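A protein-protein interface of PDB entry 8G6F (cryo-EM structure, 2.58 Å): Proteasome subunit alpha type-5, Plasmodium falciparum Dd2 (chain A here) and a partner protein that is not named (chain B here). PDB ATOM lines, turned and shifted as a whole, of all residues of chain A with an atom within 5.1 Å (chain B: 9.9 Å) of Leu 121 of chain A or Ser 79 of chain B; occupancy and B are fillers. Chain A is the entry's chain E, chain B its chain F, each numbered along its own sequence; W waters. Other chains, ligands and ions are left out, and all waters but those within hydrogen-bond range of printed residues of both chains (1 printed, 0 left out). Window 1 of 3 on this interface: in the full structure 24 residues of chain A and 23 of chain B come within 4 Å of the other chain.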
ATOM      1  N   LEU A  21      -6.160  -1.294  25.085  1.00  0.00           N
ATOM      2  CA  LEU A  21      -5.844  -2.600  24.524  1.00  0.00           C
ATOM      3  C   LEU A  21      -6.844  -3.628  25.041  1.00  0.00           C
ATOM      4  O   LEU A  21      -7.002  -3.798  26.256  1.00  0.00           O
ATOM      5  CB  LEU A  21      -4.415  -3.005  24.875  1.00  0.00           C
ATOM      6  CG  LEU A  21      -3.326  -2.072  24.344  1.00  0.00           C
ATOM      7  CD1 LEU A  21      -2.015  -2.308  25.062  1.00  0.00           C
ATOM      8  CD2 LEU A  21      -3.151  -2.255  22.853  1.00  0.00           C
ATOM      9  N   VAL A  24      -5.535  -6.224  27.480  1.00  0.00           N
ATOM     10  CA  VAL A  24      -5.297  -5.674  28.809  1.00  0.00           C
ATOM     11  C   VAL A  24      -6.609  -5.505  29.560  1.00  0.00           C
ATOM     12  O   VAL A  24      -6.693  -5.791  30.759  1.00  0.00           O
ATOM     13  CB  VAL A  24      -4.522  -4.349  28.707  1.00  0.00           C
ATOM     14  CG1 VAL A  24      -4.593  -3.595  30.019  1.00  0.00           C
ATOM     15  CG2 VAL A  24      -3.083  -4.620  28.327  1.00  0.00           C
ATOM     16  N   SER A 117       6.578  -5.089  36.087  1.00  0.00           N
ATOM     17  CA  SER A 117       5.714  -4.461  35.089  1.00  0.00           C
ATOM     18  C   SER A 117       6.285  -4.615  33.683  1.00  0.00           C
ATOM     19  O   SER A 117       5.540  -4.842  32.714  1.00  0.00           O
ATOM     20  CB  SER A 117       5.525  -2.985  35.423  1.00  0.00           C
ATOM     21  OG  SER A 117       5.358  -2.802  36.812  1.00  0.00           O
ATOM     22  N   GLU A 118       7.605  -4.469  33.553  1.00  0.00           N
ATOM     23  CA  GLU A 118       8.244  -4.634  32.255  1.00  0.00           C
ATOM     24  C   GLU A 118       7.970  -6.019  31.696  1.00  0.00           C
ATOM     25  O   GLU A 118       7.651  -6.173  30.512  1.00  0.00           O
ATOM     26  CB  GLU A 118       9.747  -4.398  32.376  1.00  0.00           C
ATOM     27  CG  GLU A 118      10.137  -2.948  32.542  1.00  0.00           C
ATOM     28  CD  GLU A 118      11.637  -2.751  32.532  1.00  0.00           C
ATOM     29  OE1 GLU A 118      12.338  -3.553  31.877  1.00  0.00           O
ATOM     30  OE2 GLU A 118      12.117  -1.796  33.180  1.00  0.00           O
ATOM     31  N   LEU A 119       8.096  -7.049  32.535  1.00  0.00           N
ATOM     32  CA  LEU A 119       7.758  -8.391  32.069  1.00  0.00           C
ATOM     33  C   LEU A 119       6.278  -8.497  31.736  1.00  0.00           C
ATOM     34  O   LEU A 119       5.901  -9.140  30.751  1.00  0.00           O
ATOM     35  CB  LEU A 119       8.138  -9.441  33.109  1.00  0.00           C
ATOM     36  CG  LEU A 119       7.892 -10.883  32.643  1.00  0.00           C
ATOM     37  CD1 LEU A 119       8.992 -11.328  31.704  1.00  0.00           C
ATOM     38  CD2 LEU A 119       7.774 -11.841  33.815  1.00  0.00           C
ATOM     39  N   ALA A 120       5.423  -7.873  32.545  1.00  0.00           N
ATOM     40  CA  ALA A 120       3.986  -8.037  32.363  1.00  0.00           C
ATOM     41  C   ALA A 120       3.542  -7.538  30.997  1.00  0.00           C
ATOM     42  O   ALA A 120       2.698  -8.163  30.344  1.00  0.00           O
ATOM     43  CB  ALA A 120       3.231  -7.306  33.470  1.00  0.00           C
ATOM     44  N   LEU A 121       4.088  -6.413  30.546  1.00  0.00           N
ATOM     45  CA  LEU A 121       3.719  -5.874  29.239  1.00  0.00           C
ATOM     46  C   LEU A 121       4.580  -6.426  28.100  1.00  0.00           C
ATOM     47  O   LEU A 121       4.663  -5.800  27.038  1.00  0.00           O
ATOM     48  CB  LEU A 121       3.776  -4.344  29.267  1.00  0.00           C
ATOM     49  CG  LEU A 121       2.413  -3.644  29.279  1.00  0.00           C
ATOM     50  CD1 LEU A 121       1.644  -3.895  27.992  1.00  0.00           C
ATOM     51  CD2 LEU A 121       1.593  -4.114  30.462  1.00  0.00           C
ATOM     52  N   ASP A 122       5.188  -7.599  28.288  1.00  0.00           N
ATOM     53  CA  ASP A 122       6.145  -8.121  27.317  1.00  0.00           C
ATOM     54  C   ASP A 122       5.496  -8.452  25.980  1.00  0.00           C
ATOM     55  O   ASP A 122       6.139  -8.323  24.934  1.00  0.00           O
ATOM     56  CB  ASP A 122       6.824  -9.367  27.884  1.00  0.00           C
ATOM     57  CG  ASP A 122       7.872  -9.936  26.954  1.00  0.00           C
ATOM     58  OD1 ASP A 122       8.342  -9.204  26.061  1.00  0.00           O
ATOM     59  OD2 ASP A 122       8.228 -11.119  27.113  1.00  0.00           O
ATOM     60  N   PHE A 123       4.240  -8.893  25.988  1.00  0.00           N
ATOM     61  CA  PHE A 123       3.613  -9.367  24.760  1.00  0.00           C
ATOM     62  C   PHE A 123       3.467  -8.270  23.715  1.00  0.00           C
ATOM     63  O   PHE A 123       3.252  -8.577  22.539  1.00  0.00           O
ATOM     64  CB  PHE A 123       2.243  -9.960  25.071  1.00  0.00           C
ATOM     65  CG  PHE A 123       1.163  -8.936  25.225  1.00  0.00           C
ATOM     66  CD1 PHE A 123       1.087  -8.158  26.364  1.00  0.00           C
ATOM     67  CD2 PHE A 123       0.227  -8.745  24.228  1.00  0.00           C
ATOM     68  CE1 PHE A 123       0.099  -7.215  26.504  1.00  0.00           C
ATOM     69  CE2 PHE A 123      -0.763  -7.802  24.366  1.00  0.00           C
ATOM     70  CZ  PHE A 123      -0.826  -7.036  25.506  1.00  0.00           C
ATOM     71  N   SER A 124       3.574  -7.002  24.111  1.00  0.00           N
ATOM     72  CA  SER A 124       3.333  -5.914  23.173  1.00  0.00           C
ATOM     73  C   SER A 124       4.387  -5.861  22.072  1.00  0.00           C
ATOM     74  O   SER A 124       4.101  -5.381  20.971  1.00  0.00           O
ATOM     75  CB  SER A 124       3.283  -4.585  23.921  1.00  0.00           C
ATOM     76  OG  SER A 124       1.955  -4.262  24.284  1.00  0.00           O
ATOM     77  N   ASN A 125       5.600  -6.339  22.345  1.00  0.00           N
ATOM     78  CA  ASN A 125       6.674  -6.358  21.354  1.00  0.00           C
ATOM     79  C   ASN A 125       7.067  -4.950  20.915  1.00  0.00           C
ATOM     80  O   ASN A 125       7.431  -4.727  19.760  1.00  0.00           O
ATOM     81  CB  ASN A 125       6.278  -7.195  20.135  1.00  0.00           C
ATOM     82  CG  ASN A 125       7.476  -7.744  19.388  1.00  0.00           C
ATOM     83  OD1 ASN A 125       8.545  -7.949  19.963  1.00  0.00           O
ATOM     84  ND2 ASN A 125       7.300  -7.992  18.097  1.00  0.00           N
ATOM     85  N   PRO A 160      -2.316  -6.022  35.497  1.00  0.00           N
ATOM     86  CA  PRO A 160      -1.977  -6.488  34.143  1.00  0.00           C
ATOM     87  C   PRO A 160      -1.674  -5.370  33.164  1.00  0.00           C
ATOM     88  O   PRO A 160      -0.908  -5.585  32.218  1.00  0.00           O
ATOM     89  CB  PRO A 160      -3.226  -7.270  33.724  1.00  0.00           C
ATOM     90  CG  PRO A 160      -3.861  -7.680  34.980  1.00  0.00           C
ATOM     91  CD  PRO A 160      -3.568  -6.617  35.985  1.00  0.00           C
ATOM     92  N   SER A 161      -2.254  -4.186  33.352  1.00  0.00           N
ATOM     93  CA  SER A 161      -2.038  -3.088  32.420  1.00  0.00           C
ATOM     94  C   SER A 161      -0.620  -2.543  32.470  1.00  0.00           C
ATOM     95  O   SER A 161      -0.262  -1.723  31.620  1.00  0.00           O
ATOM     96  CB  SER A 161      -3.029  -1.960  32.701  1.00  0.00           C
ATOM     97  OG  SER A 161      -2.673  -1.249  33.871  1.00  0.00           O
ATOM     98  N   GLY A 162       0.189  -2.970  33.434  1.00  0.00           N
ATOM     99  CA  GLY A 162       1.558  -2.527  33.546  1.00  0.00           C
ATOM    100  C   GLY A 162       1.760  -1.304  34.405  1.00  0.00           C
ATOM    101  O   GLY A 162       2.892  -0.813  34.497  1.00  0.00           O
ATOM    102  N   GLN B  60       1.077   9.382  41.174  1.00  0.00           N
ATOM    103  CA  GLN B  60       2.025   8.771  40.257  1.00  0.00           C
ATOM    104  C   GLN B  60       2.964   9.812  39.665  1.00  0.00           C
ATOM    105  O   GLN B  60       2.626  10.992  39.546  1.00  0.00           O
ATOM    106  CB  GLN B  60       1.288   8.044  39.136  1.00  0.00           C
ATOM    107  CG  GLN B  60       0.846   6.650  39.517  1.00  0.00           C
ATOM    108  CD  GLN B  60       0.173   5.927  38.379  1.00  0.00           C
ATOM    109  OE1 GLN B  60       0.301   6.315  37.220  1.00  0.00           O
ATOM    110  NE2 GLN B  60      -0.557   4.869  38.703  1.00  0.00           N
ATOM    111  N   PHE B  64      10.013  13.050  34.177  1.00  0.00           N
ATOM    112  CA  PHE B  64      11.196  12.226  34.361  1.00  0.00           C
ATOM    113  C   PHE B  64      12.411  12.917  33.763  1.00  0.00           C
ATOM    114  O   PHE B  64      12.297  13.706  32.827  1.00  0.00           O
ATOM    115  CB  PHE B  64      11.021  10.845  33.715  1.00  0.00           C
ATOM    116  CG  PHE B  64       9.705  10.202  34.020  1.00  0.00           C
ATOM    117  CD1 PHE B  64       8.586  10.493  33.264  1.00  0.00           C
ATOM    118  CD2 PHE B  64       9.582   9.307  35.062  1.00  0.00           C
ATOM    119  CE1 PHE B  64       7.380   9.904  33.544  1.00  0.00           C
ATOM    120  CE2 PHE B  64       8.374   8.718  35.345  1.00  0.00           C
ATOM    121  CZ  PHE B  64       7.273   9.016  34.586  1.00  0.00           C
ATOM    122  N   MET B  74       4.860  12.777  29.994  1.00  0.00           N
ATOM    123  CA  MET B  74       4.200  11.786  29.163  1.00  0.00           C
ATOM    124  C   MET B  74       2.694  11.900  29.328  1.00  0.00           C
ATOM    125  O   MET B  74       2.195  12.385  30.344  1.00  0.00           O
ATOM    126  CB  MET B  74       4.657  10.370  29.529  1.00  0.00           C
ATOM    127  CG  MET B  74       4.501  10.042  31.002  1.00  0.00           C
ATOM    128  SD  MET B  74       3.733   8.439  31.308  1.00  0.00           S
ATOM    129  CE  MET B  74       2.084   8.718  30.674  1.00  0.00           C
ATOM    130  N   SER B  75       1.972  11.457  28.304  1.00  0.00           N
ATOM    131  CA  SER B  75       0.528  11.296  28.406  1.00  0.00           C
ATOM    132  C   SER B  75       0.114  10.062  27.624  1.00  0.00           C
ATOM    133  O   SER B  75       0.374   9.974  26.422  1.00  0.00           O
ATOM    134  CB  SER B  75      -0.212  12.528  27.884  1.00  0.00           C
ATOM    135  OG  SER B  75      -1.575  12.488  28.254  1.00  0.00           O
ATOM    136  N   GLY B  76      -0.528   9.117  28.303  1.00  0.00           N
ATOM    137  CA  GLY B  76      -0.946   7.886  27.665  1.00  0.00           C
ATOM    138  C   GLY B  76      -0.555   6.654  28.449  1.00  0.00           C
ATOM    139  O   GLY B  76      -0.714   6.616  29.671  1.00  0.00           O
ATOM    140  N   ILE B  77      -0.031   5.643  27.763  1.00  0.00           N
ATOM    141  CA  ILE B  77       0.263   4.359  28.389  1.00  0.00           C
ATOM    142  C   ILE B  77       1.628   4.427  29.067  1.00  0.00           C
ATOM    143  O   ILE B  77       2.648   4.708  28.427  1.00  0.00           O
ATOM    144  CB  ILE B  77       0.204   3.220  27.363  1.00  0.00           C
ATOM    145  CG1 ILE B  77      -1.219   3.086  26.820  1.00  0.00           C
ATOM    146  CG2 ILE B  77       0.649   1.914  27.989  1.00  0.00           C
ATOM    147  CD1 ILE B  77      -1.339   2.177  25.627  1.00  0.00           C
ATOM    148  N   THR B  78       1.645   4.147  30.371  1.00  0.00           N
ATOM    149  CA  THR B  78       2.861   4.298  31.156  1.00  0.00           C
ATOM    150  C   THR B  78       3.939   3.305  30.744  1.00  0.00           C
ATOM    151  O   THR B  78       5.125   3.626  30.825  1.00  0.00           O
ATOM    152  CB  THR B  78       2.541   4.145  32.642  1.00  0.00           C
ATOM    153  OG1 THR B  78       1.464   5.018  32.991  1.00  0.00           O
ATOM    154  CG2 THR B  78       3.746   4.486  33.488  1.00  0.00           C
ATOM    155  N   SER B  79       3.564   2.098  30.318  1.00  0.00           N
ATOM    156  CA  SER B  79       4.572   1.143  29.869  1.00  0.00           C
ATOM    157  C   SER B  79       5.288   1.644  28.618  1.00  0.00           C
ATOM    158  O   SER B  79       6.517   1.543  28.509  1.00  0.00           O
ATOM    159  CB  SER B  79       3.928  -0.217  29.615  1.00  0.00           C
ATOM    160  OG  SER B  79       2.939  -0.135  28.606  1.00  0.00           O
ATOM    161  N   ASP B  80       4.533   2.187  27.662  1.00  0.00           N
ATOM    162  CA  ASP B  80       5.151   2.795  26.490  1.00  0.00           C
ATOM    163  C   ASP B  80       6.038   3.962  26.890  1.00  0.00           C
ATOM    164  O   ASP B  80       7.147   4.124  26.361  1.00  0.00           O
ATOM    165  CB  ASP B  80       4.074   3.269  25.518  1.00  0.00           C
ATOM    166  CG  ASP B  80       3.165   2.158  25.072  1.00  0.00           C
ATOM    167  OD1 ASP B  80       3.287   1.040  25.607  1.00  0.00           O
ATOM    168  OD2 ASP B  80       2.323   2.406  24.187  1.00  0.00           O
ATOM    169  N   ALA B  81       5.560   4.795  27.814  1.00  0.00           N
ATOM    170  CA  ALA B  81       6.373   5.912  28.272  1.00  0.00           C
ATOM    171  C   ALA B  81       7.678   5.421  28.878  1.00  0.00           C
ATOM    172  O   ALA B  81       8.733   6.019  28.661  1.00  0.00           O
ATOM    173  CB  ALA B  81       5.593   6.745  29.285  1.00  0.00           C
ATOM    174  N   LYS B  82       7.624   4.332  29.645  1.00  0.00           N
ATOM    175  CA  LYS B  82       8.832   3.779  30.249  1.00  0.00           C
ATOM    176  C   LYS B  82       9.796   3.266  29.190  1.00  0.00           C
ATOM    177  O   LYS B  82      11.008   3.487  29.287  1.00  0.00           O
ATOM    178  CB  LYS B  82       8.463   2.656  31.214  1.00  0.00           C
ATOM    179  CG  LYS B  82       7.921   3.133  32.543  1.00  0.00           C
ATOM    180  CD  LYS B  82       7.022   2.085  33.170  1.00  0.00           C
ATOM    181  CE  LYS B  82       6.478   2.533  34.514  1.00  0.00           C
ATOM    182  NZ  LYS B  82       5.237   1.800  34.883  1.00  0.00           N
ATOM    183  N   VAL B  83       9.281   2.568  28.178  1.00  0.00           N
ATOM    184  CA  VAL B  83      10.150   2.059  27.121  1.00  0.00           C
ATOM    185  C   VAL B  83      10.858   3.215  26.424  1.00  0.00           C
ATOM    186  O   VAL B  83      12.079   3.191  26.212  1.00  0.00           O
ATOM    187  CB  VAL B  83       9.341   1.210  26.124  1.00  0.00           C
ATOM    188  CG1 VAL B  83      10.109   1.025  24.829  1.00  0.00           C
ATOM    189  CG2 VAL B  83       9.000  -0.131  26.732  1.00  0.00           C
ATOM    190  N   LEU B  84      10.101   4.257  26.077  1.00  0.00           N
ATOM    191  CA  LEU B  84      10.699   5.401  25.396  1.00  0.00           C
ATOM    192  C   LEU B  84      11.679   6.139  26.298  1.00  0.00           C
ATOM    193  O   LEU B  84      12.714   6.627  25.832  1.00  0.00           O
ATOM    194  CB  LEU B  84       9.605   6.346  24.907  1.00  0.00           C
ATOM    195  CG  LEU B  84       8.763   5.806  23.753  1.00  0.00           C
ATOM    196  CD1 LEU B  84       7.534   6.664  23.552  1.00  0.00           C
ATOM    197  CD2 LEU B  84       9.581   5.737  22.481  1.00  0.00           C
ATOM    198  N   THR B  85      11.366   6.245  27.590  1.00  0.00           N
ATOM    199  CA  THR B  85      12.262   6.908  28.529  1.00  0.00           C
ATOM    200  C   THR B  85      13.589   6.172  28.627  1.00  0.00           C
ATOM    201  O   THR B  85      14.658   6.789  28.619  1.00  0.00           O
ATOM    202  CB  THR B  85      11.595   6.993  29.901  1.00  0.00           C
ATOM    203  OG1 THR B  85      10.412   7.793  29.812  1.00  0.00           O
ATOM    204  CG2 THR B  85      12.537   7.596  30.926  1.00  0.00           C
ATOM    205  N   LYS B  86      13.537   4.844  28.735  1.00  0.00           N
ATOM    206  CA  LYS B  86      14.769   4.066  28.763  1.00  0.00           C
ATOM    207  C   LYS B  86      15.557   4.254  27.478  1.00  0.00           C
ATOM    208  O   LYS B  86      16.783   4.413  27.508  1.00  0.00           O
ATOM    209  CB  LYS B  86      14.453   2.591  28.981  1.00  0.00           C
ATOM    210  CG  LYS B  86      14.157   2.229  30.421  1.00  0.00           C
ATOM    211  CD  LYS B  86      13.863   0.745  30.584  1.00  0.00           C
ATOM    212  CE  LYS B  86      15.045  -0.114  30.170  1.00  0.00           C
ATOM    213  NZ  LYS B  86      14.858  -1.542  30.535  1.00  0.00           N
ATOM    214  N   PHE B  87      14.869   4.236  26.336  1.00  0.00           N
ATOM    215  CA  PHE B  87      15.552   4.455  25.065  1.00  0.00           C
ATOM    216  C   PHE B  87      16.284   5.791  25.060  1.00  0.00           C
ATOM    217  O   PHE B  87      17.465   5.864  24.704  1.00  0.00           O
ATOM    218  CB  PHE B  87      14.542   4.388  23.921  1.00  0.00           C
ATOM    219  CG  PHE B  87      15.108   4.781  22.593  1.00  0.00           C
ATOM    220  CD1 PHE B  87      15.901   3.904  21.879  1.00  0.00           C
ATOM    221  CD2 PHE B  87      14.847   6.027  22.057  1.00  0.00           C
ATOM    222  CE1 PHE B  87      16.423   4.264  20.662  1.00  0.00           C
ATOM    223  CE2 PHE B  87      15.368   6.389  20.841  1.00  0.00           C
ATOM    224  CZ  PHE B  87      16.154   5.509  20.142  1.00  0.00           C
ATOM    225  N   LYS B 115      11.746   5.765  16.090  1.00  0.00           N
ATOM    226  CA  LYS B 115      11.315   4.617  16.878  1.00  0.00           C
ATOM    227  C   LYS B 115       9.795   4.514  16.904  1.00  0.00           C
ATOM    228  O   LYS B 115       9.235   3.418  16.803  1.00  0.00           O
ATOM    229  CB  LYS B 115      11.876   4.726  18.293  1.00  0.00           C
ATOM    230  CG  LYS B 115      11.561   3.548  19.177  1.00  0.00           C
ATOM    231  CD  LYS B 115      12.246   3.668  20.518  1.00  0.00           C
ATOM    232  CE  LYS B 115      12.138   2.385  21.312  1.00  0.00           C
ATOM    233  NZ  LYS B 115      12.756   1.240  20.601  1.00  0.00           N
ATOM    234  N   TYR B 116       9.112   5.650  17.051  1.00  0.00           N
ATOM    235  CA  TYR B 116       7.659   5.670  16.913  1.00  0.00           C
ATOM    236  C   TYR B 116       7.233   5.098  15.569  1.00  0.00           C
ATOM    237  O   TYR B 116       6.383   4.205  15.498  1.00  0.00           O
ATOM    238  CB  TYR B 116       7.142   7.102  17.036  1.00  0.00           C
ATOM    239  CG  TYR B 116       6.703   7.533  18.410  1.00  0.00           C
ATOM    240  CD1 TYR B 116       5.456   7.199  18.897  1.00  0.00           C
ATOM    241  CD2 TYR B 116       7.527   8.309  19.207  1.00  0.00           C
ATOM    242  CE1 TYR B 116       5.048   7.609  20.142  1.00  0.00           C
ATOM    243  CE2 TYR B 116       7.128   8.720  20.453  1.00  0.00           C
ATOM    244  CZ  TYR B 116       5.886   8.370  20.914  1.00  0.00           C
ATOM    245  OH  TYR B 116       5.482   8.780  22.157  1.00  0.00           O
ATOM    246  N   ARG B 126       2.381  -2.426  17.043  1.00  0.00           N
ATOM    247  CA  ARG B 126       1.359  -1.411  17.229  1.00  0.00           C
ATOM    248  C   ARG B 126       2.028  -0.097  17.592  1.00  0.00           C
ATOM    249  O   ARG B 126       3.169  -0.067  18.058  1.00  0.00           O
ATOM    250  CB  ARG B 126       0.350  -1.809  18.311  1.00  0.00           C
ATOM    251  CG  ARG B 126       0.962  -2.137  19.653  1.00  0.00           C
ATOM    252  CD  ARG B 126       0.025  -1.783  20.783  1.00  0.00           C
ATOM    253  NE  ARG B 126       0.626  -2.045  22.085  1.00  0.00           N
ATOM    254  CZ  ARG B 126       1.027  -1.118  22.944  1.00  0.00           C
ATOM    255  NH1 ARG B 126       0.911   0.173  22.682  1.00  0.00           N
ATOM    256  NH2 ARG B 126       1.561  -1.496  24.101  1.00  0.00           N
ATOM    257  N   ALA B 127       1.302   0.990  17.368  1.00  0.00           N
ATOM    258  CA  ALA B 127       1.799   2.306  17.729  1.00  0.00           C
ATOM    259  C   ALA B 127       1.887   2.446  19.243  1.00  0.00           C
ATOM    260  O   ALA B 127       1.140   1.816  19.993  1.00  0.00           O
ATOM    261  CB  ALA B 127       0.890   3.390  17.155  1.00  0.00           C
ATOM    262  N   PHE B 128       2.824   3.275  19.694  1.00  0.00           N
ATOM    263  CA  PHE B 128       2.891   3.621  21.105  1.00  0.00           C
ATOM    264  C   PHE B 128       1.694   4.484  21.476  1.00  0.00           C
ATOM    265  O   PHE B 128       1.404   5.478  20.807  1.00  0.00           O
ATOM    266  CB  PHE B 128       4.183   4.369  21.419  1.00  0.00           C
ATOM    267  CG  PHE B 128       5.425   3.555  21.234  1.00  0.00           C
ATOM    268  CD1 PHE B 128       6.006   3.432  19.989  1.00  0.00           C
ATOM    269  CD2 PHE B 128       6.022   2.928  22.308  1.00  0.00           C
ATOM    270  CE1 PHE B 128       7.152   2.690  19.819  1.00  0.00           C
ATOM    271  CE2 PHE B 128       7.167   2.187  22.142  1.00  0.00           C
ATOM    272  CZ  PHE B 128       7.733   2.069  20.895  1.00  0.00           C
ATOM    273  N   GLY B 129       1.007   4.117  22.548  1.00  0.00           N
ATOM    274  CA  GLY B 129      -0.147   4.874  22.980  1.00  0.00           C
ATOM    275  C   GLY B 129       0.225   6.011  23.903  1.00  0.00           C
ATOM    276  O   GLY B 129      -0.514   6.331  24.836  1.00  0.00           O
ATOM    277  N   VAL B 130       1.371   6.633  23.653  1.00  0.00           N
ATOM    278  CA  VAL B 130       1.915   7.656  24.534  1.00  0.00           C
ATOM    279  C   VAL B 130       2.424   8.812  23.689  1.00  0.00           C
ATOM    280  O   VAL B 130       3.059   8.607  22.650  1.00  0.00           O
ATOM    281  CB  VAL B 130       3.038   7.090  25.428  1.00  0.00           C
ATOM    282  CG1 VAL B 130       4.251   6.740  24.599  1.00  0.00           C
ATOM    283  CG2 VAL B 130       3.400   8.076  26.521  1.00  0.00           C
ATOM    284  N   LEU B 132       4.799  12.311  23.999  1.00  0.00           N
ATOM    285  CA  LEU B 132       5.894  12.793  24.829  1.00  0.00           C
ATOM    286  C   LEU B 132       6.080  14.291  24.656  1.00  0.00           C
ATOM    287  O   LEU B 132       6.005  14.811  23.540  1.00  0.00           O
ATOM    288  CB  LEU B 132       7.211  12.093  24.492  1.00  0.00           C
ATOM    289  CG  LEU B 132       7.391  10.629  24.884  1.00  0.00           C
ATOM    290  CD1 LEU B 132       8.796  10.192  24.530  1.00  0.00           C
ATOM    291  CD2 LEU B 132       7.115  10.402  26.357  1.00  0.00           C
HETATM  292  O   HOH W   1       0.924   0.627  31.052  1.00  0.00           O
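The side-chain amino group (NZ) of Lys 86 of chain B lies within salt-bridge range of the side-chain carboxylate (OE1) of Glu 118 of chain A.
The guanidinium group of Arg 126 of chain B is in hydrogen-bond range of the side-chain hydroxyl of Ser 124 of chain A, at 2.8 Å.
The side-chain carboxylate (OD1) of Asp 80 of chain B lies within hydrogen-bond range of the side-chain hydroxyl (OG) of Ser 79 of chain B (3.2 Å).
NH1 of Arg 126 of chain B is in salt-bridge range of OD2 of Asp 80 of chain B (3.0 Å).
Leu 21 of chain A touches Arg 126 of chain B (CD1 to NH2, 3.8 Å).
CG of Leu 121 of chain A touches OG of Ser 79 of chain B, at 3.6 Å.
Gly 162 of chain A touches Lys 82 of chain B.
Leu 121 of chain A touches just one residue of chain B: Ser 79 (3.6 Å).
Printed residues of chain B within 4 Å of Ser 124 of chain A: Arg 126.
Of chain B, only Lys 82 (3.5 Å) comes within 4 Å of Gly 162 of chain A.
Of the printed residues of chain A, Ser 79 of chain B touches Leu 121.
Printed residues of chain A within 4 Å of Lys 86 of chain B: Glu 118.
Of the printed residues of chain A, Arg 126 of chain B touches Leu 21 (3.8 Å) and Ser 124 (2.8 Å).
The nearest residue of chain B that does not touch Leu 121 of chain A is Arg 126 of chain B (4.6 Å).
The nearest residue of chain A that does not touch Ser 79 of chain B is Ser 161 of chain A (4.7 Å).
The nearest printed residue of chain B that does not touch Ser 124 of chain A is Asp 80 of chain B (5.6 Å).
Of the 14 printed residues of chain A, 5 touch a printed residue of chain B.
Printed residues of chain A that touch a printed residue of chain B: Leu 21, Glu 118, Leu 121, Ser 124 and Gly 162.
Water W1 bridges O of Ser 161 of chain A (2.7 Å) and N of Ser 79 of chain B (3.1 Å).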
